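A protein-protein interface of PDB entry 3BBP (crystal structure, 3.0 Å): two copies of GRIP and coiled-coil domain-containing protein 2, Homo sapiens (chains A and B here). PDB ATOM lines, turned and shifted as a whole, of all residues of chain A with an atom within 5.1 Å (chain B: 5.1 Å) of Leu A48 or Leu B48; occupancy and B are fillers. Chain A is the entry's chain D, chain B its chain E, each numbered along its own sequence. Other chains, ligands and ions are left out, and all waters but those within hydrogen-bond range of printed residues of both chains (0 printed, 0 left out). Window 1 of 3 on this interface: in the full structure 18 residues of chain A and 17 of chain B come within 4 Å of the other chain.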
ATOM      1  N   THR A  44      13.178  13.175 -23.495  1.00  0.00           N
ATOM      2  CA  THR A  44      14.629  13.031 -23.500  1.00  0.00           C
ATOM      3  C   THR A  44      15.007  11.662 -22.950  1.00  0.00           C
ATOM      4  O   THR A  44      16.039  11.098 -23.304  1.00  0.00           O
ATOM      5  CB  THR A  44      15.310  14.125 -22.655  1.00  0.00           C
ATOM      6  OG1 THR A  44      14.711  15.395 -22.940  1.00  0.00           O
ATOM      7  CG2 THR A  44      16.795  14.192 -22.971  1.00  0.00           C
ATOM      8  N   ASN A  45      14.155  11.133 -22.082  1.00  0.00           N
ATOM      9  CA  ASN A  45      14.349   9.806 -21.516  1.00  0.00           C
ATOM     10  C   ASN A  45      14.247   8.738 -22.599  1.00  0.00           C
ATOM     11  O   ASN A  45      15.014   7.775 -22.621  1.00  0.00           O
ATOM     12  CB  ASN A  45      13.302   9.546 -20.435  1.00  0.00           C
ATOM     13  CG  ASN A  45      13.807   8.632 -19.345  1.00  0.00           C
ATOM     14  OD1 ASN A  45      14.719   8.988 -18.595  1.00  0.00           O
ATOM     15  ND2 ASN A  45      13.208   7.449 -19.241  1.00  0.00           N
ATOM     16  N   ALA A  46      13.290   8.922 -23.500  1.00  0.00           N
ATOM     17  CA  ALA A  46      13.060   7.981 -24.586  1.00  0.00           C
ATOM     18  C   ALA A  46      14.271   7.875 -25.505  1.00  0.00           C
ATOM     19  O   ALA A  46      14.791   6.782 -25.732  1.00  0.00           O
ATOM     20  CB  ALA A  46      11.836   8.392 -25.376  1.00  0.00           C
ATOM     21  N   ILE A  47      14.712   9.016 -26.031  1.00  0.00           N
ATOM     22  CA  ILE A  47      15.827   9.055 -26.973  1.00  0.00           C
ATOM     23  C   ILE A  47      17.117   8.506 -26.374  1.00  0.00           C
ATOM     24  O   ILE A  47      17.983   8.012 -27.098  1.00  0.00           O
ATOM     25  CB  ILE A  47      16.088  10.483 -27.488  1.00  0.00           C
ATOM     26  CG1 ILE A  47      16.234  11.449 -26.309  1.00  0.00           C
ATOM     27  CG2 ILE A  47      14.980  10.924 -28.431  1.00  0.00           C
ATOM     28  CD1 ILE A  47      16.617  12.865 -26.699  1.00  0.00           C
ATOM     29  N   LEU A  48      17.248   8.601 -25.054  1.00  0.00           N
ATOM     30  CA  LEU A  48      18.413   8.050 -24.373  1.00  0.00           C
ATOM     31  C   LEU A  48      18.448   6.537 -24.543  1.00  0.00           C
ATOM     32  O   LEU A  48      19.459   5.974 -24.966  1.00  0.00           O
ATOM     33  CB  LEU A  48      18.406   8.412 -22.887  1.00  0.00           C
ATOM     34  CG  LEU A  48      18.711   9.862 -22.501  1.00  0.00           C
ATOM     35  CD1 LEU A  48      18.774   9.999 -20.991  1.00  0.00           C
ATOM     36  CD2 LEU A  48      20.008  10.332 -23.132  1.00  0.00           C
ATOM     37  N   MET A  49      17.335   5.885 -24.222  1.00  0.00           N
ATOM     38  CA  MET A  49      17.247   4.435 -24.345  1.00  0.00           C
ATOM     39  C   MET A  49      17.419   3.960 -25.784  1.00  0.00           C
ATOM     40  O   MET A  49      17.882   2.844 -26.024  1.00  0.00           O
ATOM     41  CB  MET A  49      15.934   3.918 -23.759  1.00  0.00           C
ATOM     42  CG  MET A  49      15.958   3.774 -22.248  1.00  0.00           C
ATOM     43  SD  MET A  49      14.336   3.442 -21.547  1.00  0.00           S
ATOM     44  CE  MET A  49      13.420   4.866 -22.148  1.00  0.00           C
ATOM     45  N   GLU A  50      17.049   4.809 -26.739  1.00  0.00           N
ATOM     46  CA  GLU A  50      17.248   4.499 -28.150  1.00  0.00           C
ATOM     47  C   GLU A  50      18.732   4.492 -28.490  1.00  0.00           C
ATOM     48  O   GLU A  50      19.219   3.582 -29.158  1.00  0.00           O
ATOM     49  CB  GLU A  50      16.505   5.499 -29.040  1.00  0.00           C
ATOM     50  CG  GLU A  50      15.009   5.253 -29.147  1.00  0.00           C
ATOM     51  CD  GLU A  50      14.303   6.325 -29.959  1.00  0.00           C
ATOM     52  OE1 GLU A  50      14.995   7.108 -30.644  1.00  0.00           O
ATOM     53  OE2 GLU A  50      13.057   6.385 -29.910  1.00  0.00           O
ATOM     54  N   GLN A  51      19.449   5.511 -28.024  1.00  0.00           N
ATOM     55  CA  GLN A  51      20.888   5.596 -28.247  1.00  0.00           C
ATOM     56  C   GLN A  51      21.601   4.435 -27.566  1.00  0.00           C
ATOM     57  O   GLN A  51      22.581   3.904 -28.086  1.00  0.00           O
ATOM     58  CB  GLN A  51      21.443   6.926 -27.732  1.00  0.00           C
ATOM     59  CG  GLN A  51      22.930   7.118 -28.002  1.00  0.00           C
ATOM     60  CD  GLN A  51      23.484   8.368 -27.351  1.00  0.00           C
ATOM     61  OE1 GLN A  51      22.739   9.158 -26.769  1.00  0.00           O
ATOM     62  NE2 GLN A  51      24.796   8.556 -27.447  1.00  0.00           N
ATOM     63  N   ILE A  52      21.101   4.047 -26.399  1.00  0.00           N
ATOM     64  CA  ILE A  52      21.669   2.927 -25.657  1.00  0.00           C
ATOM     65  C   ILE A  52      21.566   1.621 -26.441  1.00  0.00           C
ATOM     66  O   ILE A  52      22.527   0.861 -26.520  1.00  0.00           O
ATOM     67  CB  ILE A  52      20.994   2.753 -24.283  1.00  0.00           C
ATOM     68  CG1 ILE A  52      21.347   3.921 -23.367  1.00  0.00           C
ATOM     69  CG2 ILE A  52      21.433   1.460 -23.640  1.00  0.00           C
ATOM     70  CD1 ILE A  52      20.725   3.822 -22.000  1.00  0.00           C
ATOM     71  N   THR B  44      16.385   8.513 -12.972  1.00  0.00           N
ATOM     72  CA  THR B  44      16.550   7.465 -13.973  1.00  0.00           C
ATOM     73  C   THR B  44      17.240   8.034 -15.204  1.00  0.00           C
ATOM     74  O   THR B  44      17.942   7.325 -15.925  1.00  0.00           O
ATOM     75  CB  THR B  44      15.197   6.862 -14.389  1.00  0.00           C
ATOM     76  OG1 THR B  44      14.392   6.630 -13.227  1.00  0.00           O
ATOM     77  CG2 THR B  44      15.410   5.549 -15.122  1.00  0.00           C
ATOM     78  N   ASN B  45      17.033   9.324 -15.437  1.00  0.00           N
ATOM     79  CA  ASN B  45      17.675  10.028 -16.536  1.00  0.00           C
ATOM     80  C   ASN B  45      19.189  10.083 -16.342  1.00  0.00           C
ATOM     81  O   ASN B  45      19.956   9.923 -17.290  1.00  0.00           O
ATOM     82  CB  ASN B  45      17.118  11.447 -16.636  1.00  0.00           C
ATOM     83  CG  ASN B  45      17.112  11.972 -18.052  1.00  0.00           C
ATOM     84  OD1 ASN B  45      16.388  11.460 -18.909  1.00  0.00           O
ATOM     85  ND2 ASN B  45      17.909  13.007 -18.306  1.00  0.00           N
ATOM     86  N   ALA B  46      19.607  10.312 -15.101  1.00  0.00           N
ATOM     87  CA  ALA B  46      21.022  10.399 -14.757  1.00  0.00           C
ATOM     88  C   ALA B  46      21.763   9.093 -15.031  1.00  0.00           C
ATOM     89  O   ALA B  46      22.774   9.081 -15.736  1.00  0.00           O
ATOM     90  CB  ALA B  46      21.185  10.796 -13.296  1.00  0.00           C
ATOM     91  N   ILE B  47      21.258   8.000 -14.463  1.00  0.00           N
ATOM     92  CA  ILE B  47      21.886   6.687 -14.603  1.00  0.00           C
ATOM     93  C   ILE B  47      21.947   6.214 -16.052  1.00  0.00           C
ATOM     94  O   ILE B  47      22.826   5.435 -16.422  1.00  0.00           O
ATOM     95  CB  ILE B  47      21.157   5.613 -13.773  1.00  0.00           C
ATOM     96  CG1 ILE B  47      19.662   5.603 -14.110  1.00  0.00           C
ATOM     97  CG2 ILE B  47      21.388   5.843 -12.294  1.00  0.00           C
ATOM     98  CD1 ILE B  47      18.873   4.487 -13.441  1.00  0.00           C
ATOM     99  N   LEU B  48      21.004   6.670 -16.869  1.00  0.00           N
ATOM    100  CA  LEU B  48      21.034   6.357 -18.291  1.00  0.00           C
ATOM    101  C   LEU B  48      22.299   6.926 -18.927  1.00  0.00           C
ATOM    102  O   LEU B  48      23.048   6.205 -19.584  1.00  0.00           O
ATOM    103  CB  LEU B  48      19.792   6.899 -19.004  1.00  0.00           C
ATOM    104  CG  LEU B  48      18.455   6.200 -18.730  1.00  0.00           C
ATOM    105  CD1 LEU B  48      17.360   6.789 -19.603  1.00  0.00           C
ATOM    106  CD2 LEU B  48      18.554   4.700 -18.955  1.00  0.00           C
ATOM    107  N   MET B  49      22.540   8.219 -18.718  1.00  0.00           N
ATOM    108  CA  MET B  49      23.705   8.879 -19.298  1.00  0.00           C
ATOM    109  C   MET B  49      25.013   8.292 -18.782  1.00  0.00           C
ATOM    110  O   MET B  49      26.030   8.322 -19.472  1.00  0.00           O
ATOM    111  CB  MET B  49      23.654  10.390 -19.061  1.00  0.00           C
ATOM    112  CG  MET B  49      22.758  11.135 -20.043  1.00  0.00           C
ATOM    113  SD  MET B  49      22.472  12.849 -19.574  1.00  0.00           S
ATOM    114  CE  MET B  49      21.775  12.640 -17.935  1.00  0.00           C
ATOM    115  N   GLU B  50      24.982   7.757 -17.566  1.00  0.00           N
ATOM    116  CA  GLU B  50      26.146   7.085 -17.003  1.00  0.00           C
ATOM    117  C   GLU B  50      26.436   5.796 -17.754  1.00  0.00           C
ATOM    118  O   GLU B  50      27.583   5.524 -18.103  1.00  0.00           O
ATOM    119  CB  GLU B  50      25.945   6.792 -15.517  1.00  0.00           C
ATOM    120  CG  GLU B  50      26.143   7.998 -14.613  1.00  0.00           C
ATOM    121  CD  GLU B  50      25.846   7.683 -13.159  1.00  0.00           C
ATOM    122  OE1 GLU B  50      25.729   6.483 -12.821  1.00  0.00           O
ATOM    123  OE2 GLU B  50      25.730   8.633 -12.354  1.00  0.00           O
ATOM    124  N   GLN B  51      25.394   5.007 -18.004  1.00  0.00           N
ATOM    125  CA  GLN B  51      25.533   3.764 -18.758  1.00  0.00           C
ATOM    126  C   GLN B  51      25.995   4.053 -20.181  1.00  0.00           C
ATOM    127  O   GLN B  51      26.780   3.296 -20.754  1.00  0.00           O
ATOM    128  CB  GLN B  51      24.213   2.986 -18.782  1.00  0.00           C
ATOM    129  CG  GLN B  51      24.296   1.634 -19.493  1.00  0.00           C
ATOM    130  CD  GLN B  51      22.945   0.948 -19.615  1.00  0.00           C
ATOM    131  OE1 GLN B  51      21.943   1.437 -19.095  1.00  0.00           O
ATOM    132  NE2 GLN B  51      22.914  -0.190 -20.304  1.00  0.00           N
ATOM    133  N   ILE B  52      25.509   5.157 -20.738  1.00  0.00           N
ATOM    134  CA  ILE B  52      25.880   5.562 -22.089  1.00  0.00           C
ATOM    135  C   ILE B  52      27.373   5.855 -22.185  1.00  0.00           C
ATOM    136  O   ILE B  52      28.041   5.418 -23.122  1.00  0.00           O
ATOM    137  CB  ILE B  52      25.079   6.793 -22.554  1.00  0.00           C
ATOM    138  CG1 ILE B  52      23.613   6.416 -22.773  1.00  0.00           C
ATOM    139  CG2 ILE B  52      25.667   7.359 -23.829  1.00  0.00           C
ATOM    140  CD1 ILE B  52      22.750   7.573 -23.212  1.00  0.00           C
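OD1 of Asn B45 sits close to OD1 of Asn A45.
Glu A50 touches none of the printed residues of chain B.
Printed residues of chain B within 4 Å of Gln A51: Ile B52 (3.9 Å).
Of the printed residues of chain B, Ile A52 touches Leu B48, Gln B51 and Ile B52.
Printed residues of chain A within 4 Å of Asn B45: Asn A45 (3.0 Å) and Leu A48 (3.5 Å).
Leu B48 touches just these residues of chain A: Asn A45 (3.6 Å), Leu A48 (3.8 Å) and Ile A52 (3.8 Å).
Of the printed residues of chain A, Gln B51 touches Ile A52 (3.95 Å).
Printed residues of chain A within 4 Å of Ile B52: Leu A48, Gln A51 and Ile A52.
The nearest residue of chain A that does not touch Leu B48 is Met A49 (4.2 Å).
Asn A45 touches Leu B48 (OD1 to CD1, 3.6 Å).
Leu A48 touches Asn B45 (CD1 to OD1, 3.5 Å).
Leu B48 touches Leu A48.
CD2 of Leu A48 touches CD1 of Ile B52, at 3.9 Å.
Gln A51 touches Ile B52.
Leu B48 touches Ile A52 (CD2 to CD1, 3.8 Å).
Ile A52 touches Gln B51 (CD1 to OE1, 3.95 Å).
Ile A52 touches Ile B52 (CG1 to CG1, 3.4 Å).
Leu A48 touches its own counterpart, Leu B48.
Leu A48 touches Ile B52, and with the chains exchanged Ile A52 touches Leu B48.
Gln A51 touches Ile B52, and with the chains exchanged Ile A52 touches Gln B51.
Ile B52 touches its own counterpart, Ile A52.
Of the 9 printed residues of chain A, 4 touch a printed residue of chain B.
Hydrophobic or aromatic side chains of chain A within 4 Å of the printed part of chain B: Leu A48 and Ile A52.
Among the printed residues, no Asp or Glu carboxylate lies within 4 Å of a Lys or Arg side-chain nitrogen of the other chain.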
